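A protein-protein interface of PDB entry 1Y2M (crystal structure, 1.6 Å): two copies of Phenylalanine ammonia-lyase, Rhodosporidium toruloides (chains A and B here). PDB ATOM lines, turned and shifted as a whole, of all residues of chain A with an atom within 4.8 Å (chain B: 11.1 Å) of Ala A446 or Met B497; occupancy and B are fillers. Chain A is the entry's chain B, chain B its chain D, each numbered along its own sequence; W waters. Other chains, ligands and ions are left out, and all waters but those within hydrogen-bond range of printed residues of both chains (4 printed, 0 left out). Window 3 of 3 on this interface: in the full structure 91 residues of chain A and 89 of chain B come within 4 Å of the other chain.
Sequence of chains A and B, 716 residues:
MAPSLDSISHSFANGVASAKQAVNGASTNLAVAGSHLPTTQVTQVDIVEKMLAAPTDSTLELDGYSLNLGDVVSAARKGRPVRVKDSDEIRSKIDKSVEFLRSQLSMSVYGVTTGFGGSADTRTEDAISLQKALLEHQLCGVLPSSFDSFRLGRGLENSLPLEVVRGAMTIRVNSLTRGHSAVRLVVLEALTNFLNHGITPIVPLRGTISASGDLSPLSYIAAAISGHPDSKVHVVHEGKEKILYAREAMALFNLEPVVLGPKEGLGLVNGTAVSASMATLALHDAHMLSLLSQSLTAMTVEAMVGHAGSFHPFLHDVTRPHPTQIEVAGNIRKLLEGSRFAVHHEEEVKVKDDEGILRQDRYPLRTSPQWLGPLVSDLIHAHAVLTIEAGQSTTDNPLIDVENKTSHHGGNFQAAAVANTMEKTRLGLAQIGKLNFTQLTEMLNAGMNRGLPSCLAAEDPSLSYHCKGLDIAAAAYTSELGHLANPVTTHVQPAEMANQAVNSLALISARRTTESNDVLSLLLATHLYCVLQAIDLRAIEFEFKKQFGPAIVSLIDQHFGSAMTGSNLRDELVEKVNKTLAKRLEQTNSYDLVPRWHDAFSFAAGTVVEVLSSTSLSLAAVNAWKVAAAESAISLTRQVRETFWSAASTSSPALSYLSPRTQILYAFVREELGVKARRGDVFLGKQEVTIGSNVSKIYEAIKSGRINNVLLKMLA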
ATOM      1  N   THR A 441      -1.061 -13.625  14.178  1.00  0.00           N
ATOM      2  CA  THR A 441      -0.725 -15.048  14.077  1.00  0.00           C
ATOM      3  C   THR A 441      -1.253 -15.821  15.296  1.00  0.00           C
ATOM      4  O   THR A 441      -1.599 -17.000  15.207  1.00  0.00           O
ATOM      5  CB  THR A 441       0.751 -15.235  13.756  1.00  0.00           C
ATOM      6  OG1 THR A 441       0.940 -16.571  13.206  1.00  0.00           O
ATOM      7  CG2 THR A 441       1.604 -15.004  14.960  1.00  0.00           C
ATOM      8  N   LEU A 444      -4.891 -16.447  14.468  1.00  0.00           N
ATOM      9  CA  LEU A 444      -5.006 -17.487  13.443  1.00  0.00           C
ATOM     10  C   LEU A 444      -4.530 -18.873  13.911  1.00  0.00           C
ATOM     11  O   LEU A 444      -4.468 -19.836  13.103  1.00  0.00           O
ATOM     12  CB  LEU A 444      -4.228 -17.063  12.200  1.00  0.00           C
ATOM     13  CG  LEU A 444      -4.766 -15.775  11.547  1.00  0.00           C
ATOM     14  CD1 LEU A 444      -3.958 -15.515  10.242  1.00  0.00           C
ATOM     15  CD2 LEU A 444      -6.237 -15.780  11.339  1.00  0.00           C
ATOM     16  N   ASN A 445      -4.152 -18.964  15.176  1.00  0.00           N
ATOM     17  CA  ASN A 445      -3.718 -20.223  15.797  1.00  0.00           C
ATOM     18  C   ASN A 445      -4.829 -20.833  16.616  1.00  0.00           C
ATOM     19  O   ASN A 445      -5.212 -20.303  17.657  1.00  0.00           O
ATOM     20  CB  ASN A 445      -2.478 -19.947  16.668  1.00  0.00           C
ATOM     21  CG  ASN A 445      -1.814 -21.220  17.169  1.00  0.00           C
ATOM     22  OD1 ASN A 445      -2.495 -22.155  17.588  1.00  0.00           O
ATOM     23  ND2 ASN A 445      -0.493 -21.273  17.122  1.00  0.00           N
ATOM     24  N   ALA A 446      -5.344 -21.963  16.131  1.00  0.00           N
ATOM     25  CA  ALA A 446      -6.517 -22.622  16.742  1.00  0.00           C
ATOM     26  C   ALA A 446      -6.260 -23.000  18.185  1.00  0.00           C
ATOM     27  O   ALA A 446      -7.167 -23.041  18.998  1.00  0.00           O
ATOM     28  CB  ALA A 446      -6.862 -23.899  15.933  1.00  0.00           C
ATOM     29  N   GLY A 447      -5.008 -23.295  18.488  1.00  0.00           N
ATOM     30  CA  GLY A 447      -4.606 -23.610  19.843  1.00  0.00           C
ATOM     31  C   GLY A 447      -4.537 -22.442  20.775  1.00  0.00           C
ATOM     32  O   GLY A 447      -4.508 -22.641  21.966  1.00  0.00           O
ATOM     33  N   MET A 448      -4.530 -21.218  20.250  1.00  0.00           N
ATOM     34  CA  MET A 448      -4.357 -20.021  21.089  1.00  0.00           C
ATOM     35  C   MET A 448      -5.513 -19.018  21.039  1.00  0.00           C
ATOM     36  O   MET A 448      -5.493 -18.067  21.766  1.00  0.00           O
ATOM     37  CB  MET A 448      -3.091 -19.270  20.637  1.00  0.00           C
ATOM     38  CG  MET A 448      -1.883 -20.098  20.662  1.00  0.00           C
ATOM     39  SD  MET A 448      -0.271 -19.186  19.890  1.00  0.00           S
ATOM     40  CE  MET A 448      -0.008 -18.043  21.337  1.00  0.00           C
ATOM     41  N   ASN A 449      -6.464 -19.172  20.114  1.00  0.00           N
ATOM     42  CA  ASN A 449      -7.410 -18.112  19.756  1.00  0.00           C
ATOM     43  C   ASN A 449      -8.764 -18.194  20.418  1.00  0.00           C
ATOM     44  O   ASN A 449      -9.770 -17.688  19.941  1.00  0.00           O
ATOM     45  CB  ASN A 449      -7.493 -18.023  18.218  1.00  0.00           C
ATOM     46  CG  ASN A 449      -8.117 -19.242  17.595  1.00  0.00           C
ATOM     47  OD1 ASN A 449      -8.549 -20.156  18.303  1.00  0.00           O
ATOM     48  ND2 ASN A 449      -8.172 -19.281  16.263  1.00  0.00           N
ATOM     49  N   SER A 454     -10.700 -22.835  13.268  1.00  0.00           N
ATOM     50  CA  SER A 454      -9.407 -23.031  12.582  1.00  0.00           C
ATOM     51  C   SER A 454      -9.339 -22.227  11.280  1.00  0.00           C
ATOM     52  O   SER A 454     -10.284 -22.241  10.468  1.00  0.00           O
ATOM     53  CB  SER A 454      -9.166 -24.497  12.238  1.00  0.00           C
ATOM     54  OG  SER A 454     -10.318 -24.978  11.592  1.00  0.00           O
ATOM     55  N   ASP A 471      -1.758 -15.924   7.068  1.00  0.00           N
ATOM     56  CA  ASP A 471      -0.838 -16.117   8.196  1.00  0.00           C
ATOM     57  C   ASP A 471       0.585 -16.143   7.655  1.00  0.00           C
ATOM     58  O   ASP A 471       1.476 -15.477   8.153  1.00  0.00           O
ATOM     59  CB  ASP A 471      -1.179 -17.459   8.877  1.00  0.00           C
ATOM     60  CG  ASP A 471      -0.651 -17.568  10.293  1.00  0.00           C
ATOM     61  OD1 ASP A 471      -0.375 -16.533  10.971  1.00  0.00           O
ATOM     62  OD2 ASP A 471      -0.590 -18.735  10.781  1.00  0.00           O
ATOM     63  N   GLU A 586     -13.543 -25.099  23.332  1.00  0.00           N
ATOM     64  CA  GLU A 586     -12.416 -24.175  23.044  1.00  0.00           C
ATOM     65  C   GLU A 586     -11.287 -24.896  22.332  1.00  0.00           C
ATOM     66  O   GLU A 586     -10.503 -24.290  21.600  1.00  0.00           O
ATOM     67  CB  GLU A 586     -11.897 -23.532  24.329  1.00  0.00           C
ATOM     68  CG  GLU A 586     -10.644 -22.686  24.124  1.00  0.00           C
ATOM     69  CD  GLU A 586     -10.421 -21.589  25.184  1.00  0.00           C
ATOM     70  OE1 GLU A 586     -11.386 -21.190  25.884  1.00  0.00           O
ATOM     71  OE2 GLU A 586      -9.260 -21.107  25.272  1.00  0.00           O
ATOM     72  N   ASN A 589     -11.888 -26.613  18.032  1.00  0.00           N
ATOM     73  CA  ASN A 589     -12.195 -25.646  17.011  1.00  0.00           C
ATOM     74  C   ASN A 589     -11.626 -25.995  15.608  1.00  0.00           C
ATOM     75  O   ASN A 589     -11.926 -25.291  14.635  1.00  0.00           O
ATOM     76  CB  ASN A 589     -11.819 -24.218  17.462  1.00  0.00           C
ATOM     77  CG  ASN A 589     -10.359 -24.105  17.994  1.00  0.00           C
ATOM     78  OD1 ASN A 589      -9.767 -25.092  18.485  1.00  0.00           O
ATOM     79  ND2 ASN A 589      -9.776 -22.885  17.892  1.00  0.00           N
ATOM     80  N   SER A 590     -10.871 -27.109  15.514  1.00  0.00           N
ATOM     81  CA  SER A 590     -10.441 -27.660  14.218  1.00  0.00           C
ATOM     82  C   SER A 590     -11.246 -28.862  13.776  1.00  0.00           C
ATOM     83  O   SER A 590     -10.915 -29.421  12.757  1.00  0.00           O
ATOM     84  CB  SER A 590      -8.966 -28.056  14.230  1.00  0.00           C
ATOM     85  OG  SER A 590      -8.181 -26.930  14.616  1.00  0.00           O
ATOM     86  N   ILE B 209       7.072 -17.011   2.004  1.00  0.00           N
ATOM     87  CA  ILE B 209       8.237 -17.243   2.849  1.00  0.00           C
ATOM     88  C   ILE B 209       9.169 -18.327   2.249  1.00  0.00           C
ATOM     89  O   ILE B 209      10.169 -18.657   2.876  1.00  0.00           O
ATOM     90  CB  ILE B 209       7.849 -17.576   4.323  1.00  0.00           C
ATOM     91  CG1 ILE B 209       7.033 -18.858   4.421  1.00  0.00           C
ATOM     92  CG2 ILE B 209       7.123 -16.422   4.943  1.00  0.00           C
ATOM     93  CD1 ILE B 209       6.556 -19.148   5.839  1.00  0.00           C
ATOM     94  N   GLN B 493      10.326 -15.656  10.740  1.00  0.00           N
ATOM     95  CA  GLN B 493       9.216 -15.606  11.650  1.00  0.00           C
ATOM     96  C   GLN B 493       8.535 -16.963  11.811  1.00  0.00           C
ATOM     97  O   GLN B 493       8.622 -17.801  10.931  1.00  0.00           O
ATOM     98  CB  GLN B 493       8.184 -14.625  11.130  1.00  0.00           C
ATOM     99  CG  GLN B 493       8.695 -13.222  10.905  1.00  0.00           C
ATOM    100  CD  GLN B 493       9.194 -12.561  12.185  1.00  0.00           C
ATOM    101  OE1 GLN B 493       8.526 -12.592  13.206  1.00  0.00           O
ATOM    102  NE2 GLN B 493      10.427 -12.011  12.150  1.00  0.00           N
ATOM    103  N   PRO B 494       7.869 -17.204  12.949  1.00  0.00           N
ATOM    104  CA  PRO B 494       7.204 -18.504  13.195  1.00  0.00           C
ATOM    105  C   PRO B 494       5.921 -18.739  12.462  1.00  0.00           C
ATOM    106  O   PRO B 494       4.843 -18.825  13.070  1.00  0.00           O
ATOM    107  CB  PRO B 494       6.917 -18.443  14.679  1.00  0.00           C
ATOM    108  CG  PRO B 494       6.706 -16.999  14.928  1.00  0.00           C
ATOM    109  CD  PRO B 494       7.774 -16.327  14.118  1.00  0.00           C
ATOM    110  N   ALA B 495       6.032 -18.954  11.179  1.00  0.00           N
ATOM    111  CA  ALA B 495       4.871 -18.945  10.344  1.00  0.00           C
ATOM    112  C   ALA B 495       3.947 -20.167  10.463  1.00  0.00           C
ATOM    113  O   ALA B 495       4.394 -21.309  10.652  1.00  0.00           O
ATOM    114  CB  ALA B 495       5.299 -18.670   8.872  1.00  0.00           C
ATOM    115  N   GLU B 496       2.650 -19.922  10.276  1.00  0.00           N
ATOM    116  CA  GLU B 496       1.656 -20.956  10.140  1.00  0.00           C
ATOM    117  C   GLU B 496       1.552 -21.856  11.354  1.00  0.00           C
ATOM    118  O   GLU B 496       1.785 -23.056  11.307  1.00  0.00           O
ATOM    119  CB  GLU B 496       1.903 -21.800   8.863  1.00  0.00           C
ATOM    120  CG  GLU B 496       0.673 -22.584   8.434  1.00  0.00           C
ATOM    121  CD  GLU B 496       0.910 -24.061   8.175  1.00  0.00           C
ATOM    122  OE1 GLU B 496       1.907 -24.500   7.520  1.00  0.00           O
ATOM    123  OE2 GLU B 496       0.033 -24.808   8.614  1.00  0.00           O
ATOM    124  N   MET B 497       1.192 -21.250  12.485  1.00  0.00           N
ATOM    125  CA  MET B 497       1.069 -21.982  13.737  1.00  0.00           C
ATOM    126  C   MET B 497       2.376 -22.667  14.138  1.00  0.00           C
ATOM    127  O   MET B 497       2.367 -23.702  14.823  1.00  0.00           O
ATOM    128  CB  MET B 497      -0.082 -22.976  13.733  1.00  0.00           C
ATOM    129  CG  MET B 497      -1.385 -22.261  13.565  1.00  0.00           C
ATOM    130  SD  MET B 497      -2.882 -23.592  13.589  1.00  0.00           S
ATOM    131  CE  MET B 497      -2.563 -24.516  15.219  1.00  0.00           C
ATOM    132  N   ALA B 498       3.483 -22.040  13.727  1.00  0.00           N
ATOM    133  CA  ALA B 498       4.812 -22.616  13.909  1.00  0.00           C
ATOM    134  C   ALA B 498       5.026 -23.944  13.197  1.00  0.00           C
ATOM    135  O   ALA B 498       6.096 -24.567  13.367  1.00  0.00           O
ATOM    136  CB  ALA B 498       5.198 -22.731  15.365  1.00  0.00           C
ATOM    137  N   ASN B 499       4.113 -24.385  12.315  1.00  0.00           N
ATOM    138  CA  ASN B 499       4.437 -25.532  11.465  1.00  0.00           C
ATOM    139  C   ASN B 499       5.628 -25.191  10.556  1.00  0.00           C
ATOM    140  O   ASN B 499       6.550 -26.015  10.322  1.00  0.00           O
ATOM    141  CB  ASN B 499       3.251 -26.012  10.639  1.00  0.00           C
ATOM    142  CG  ASN B 499       3.633 -27.209   9.708  1.00  0.00           C
ATOM    143  OD1 ASN B 499       4.137 -28.236  10.171  1.00  0.00           O
ATOM    144  ND2 ASN B 499       3.346 -27.070   8.383  1.00  0.00           N
ATOM    145  N   GLN B 500       5.636 -23.927  10.106  1.00  0.00           N
ATOM    146  CA  GLN B 500       6.671 -23.399   9.270  1.00  0.00           C
ATOM    147  C   GLN B 500       7.621 -22.514  10.070  1.00  0.00           C
ATOM    148  O   GLN B 500       7.990 -21.411   9.659  1.00  0.00           O
ATOM    149  CB  GLN B 500       6.105 -22.697   8.037  1.00  0.00           C
ATOM    150  CG  GLN B 500       5.035 -23.500   7.277  1.00  0.00           C
ATOM    151  CD  GLN B 500       4.759 -23.045   5.877  1.00  0.00           C
ATOM    152  OE1 GLN B 500       5.609 -22.429   5.220  1.00  0.00           O
ATOM    153  NE2 GLN B 500       3.560 -23.384   5.366  1.00  0.00           N
ATOM    154  N   ALA B 501       8.025 -23.003  11.241  1.00  0.00           N
ATOM    155  CA  ALA B 501       8.812 -22.176  12.160  1.00  0.00           C
ATOM    156  C   ALA B 501      10.220 -21.782  11.627  1.00  0.00           C
ATOM    157  O   ALA B 501      10.831 -20.801  12.088  1.00  0.00           O
ATOM    158  CB  ALA B 501       8.937 -22.853  13.478  1.00  0.00           C
ATOM    159  N   VAL B 502      10.736 -22.617  10.721  1.00  0.00           N
ATOM    160  CA  VAL B 502      11.871 -22.264   9.873  1.00  0.00           C
ATOM    161  C   VAL B 502      11.357 -22.189   8.426  1.00  0.00           C
ATOM    162  O   VAL B 502      10.616 -23.052   7.958  1.00  0.00           O
ATOM    163  CB  VAL B 502      13.054 -23.240   9.927  1.00  0.00           C
ATOM    164  CG1 VAL B 502      13.857 -23.025  11.199  1.00  0.00           C
ATOM    165  CG2 VAL B 502      12.638 -24.659   9.803  1.00  0.00           C
ATOM    166  N   ASN B 503      11.736 -21.116   7.748  1.00  0.00           N
ATOM    167  CA  ASN B 503      11.337 -20.831   6.393  1.00  0.00           C
ATOM    168  C   ASN B 503      12.474 -20.035   5.741  1.00  0.00           C
ATOM    169  O   ASN B 503      13.160 -19.252   6.407  1.00  0.00           O
ATOM    170  CB  ASN B 503       9.963 -20.156   6.333  1.00  0.00           C
ATOM    171  CG  ASN B 503       9.852 -18.933   7.241  1.00  0.00           C
ATOM    172  OD1 ASN B 503      10.304 -17.845   6.883  1.00  0.00           O
ATOM    173  ND2 ASN B 503       9.212 -19.102   8.381  1.00  0.00           N
HETATM  174  O   HOH W   1      -6.183 -22.044  13.008  1.00  0.00           O
HETATM  175  O   HOH W   2       2.756 -18.295  14.292  1.00  0.00           O
HETATM  176  O   HOH W   3      -0.925 -19.054  13.267  1.00  0.00           O
HETATM  177  O   HOH W   4       2.499 -16.837  10.436  1.00  0.00           O
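OD2 of Asp A471 lies close to N of Glu B496, at 3.5 Å.
OD1 of Asp A471 is in hydrogen-bond range of OG1 of Thr A441 (2.6 Å). The side-chain amide oxygen (OD1) of Asn A445 sits at hydrogen-bond distance from the backbone NH (N) of Gly A447 (2.9 Å). ND2 of Asn A445 is in hydrogen-bond range of SD of Met A448. OD1 of Asn A449 lies close to O of Ala A446, at 3.3 Å. O of Ala A446 sits at hydrogen-bond distance from ND2 of Asn A589 (2.8 Å). OE1 of Glu B496 is in hydrogen-bond range of NE2 of Gln B500.
Among the printed residues, pairs that only touch across the chains: Leu A444 with Met B497 (3.9 Å), Asn A445 with Met B497 (3.3 Å), Ala A446 with Met B497 (3.9 Å) and Asp A471 with Met B497 (3.5 Å).
Of the printed residues of chain B, Leu A444 touches Met B497 (3.9 Å). Of chain B, only Met B497 (3.3 Å) comes within 4 Å of Asn A445. Of chain B, only Met B497 (3.9 Å) comes within 4 Å of Ala A446. No residue of chain B comes within 4 Å of Asn A449. No residue of chain B comes within 4 Å of Ser A454. Of the printed residues of chain B, Asp A471 touches Glu B496 and Met B497. No residue of chain B comes within 4 Å of Asn A589. Printed residues of chain A within 4 Å of Glu B496: Asp A471. Met B497 touches four residues of chain A. Val B502 touches none of the printed residues of chain A. The nearest printed residue of chain B that does not touch Leu A444 is Glu B496 (6.6 Å).
Along chain B the printed residues that touch a printed residue of chain A span positions 496 to 497. Of the 12 printed residues of chain A, 4 touch a printed residue of chain B. Among the printed residues, no Asp or Glu carboxylate lies within 4 Å of a Lys or Arg side-chain nitrogen of the other chain.
No position is printed for both chains. Of the 5 pairs that touch across the chains among the printed residues, none has its exchanged pair printed and touching as well.
Water W2 lies within hydrogen-bond range of O of Pro B494 (2.5 Å) and OG1 of Thr A441 (2.7 Å). Water W3 lies within hydrogen-bond range of the side-chain carboxylate (OD2) of Asp A471 (2.5 Å), the backbone carbonyl oxygen (O) of Thr A441 (2.9 Å) and the backbone NH (N) of Met B497 (3.1 Å). Water W1 lies within hydrogen-bond range of the backbone carbonyl oxygen of Leu A444, the backbone NH of Ala A446 and the side-chain sulfur of Met B497. Water W4 lies within hydrogen-bond range of O of Asp A471 (2.8 Å), N of Glu B496 (3.1 Å) and OG1 of Thr A441 (3.2 Å).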
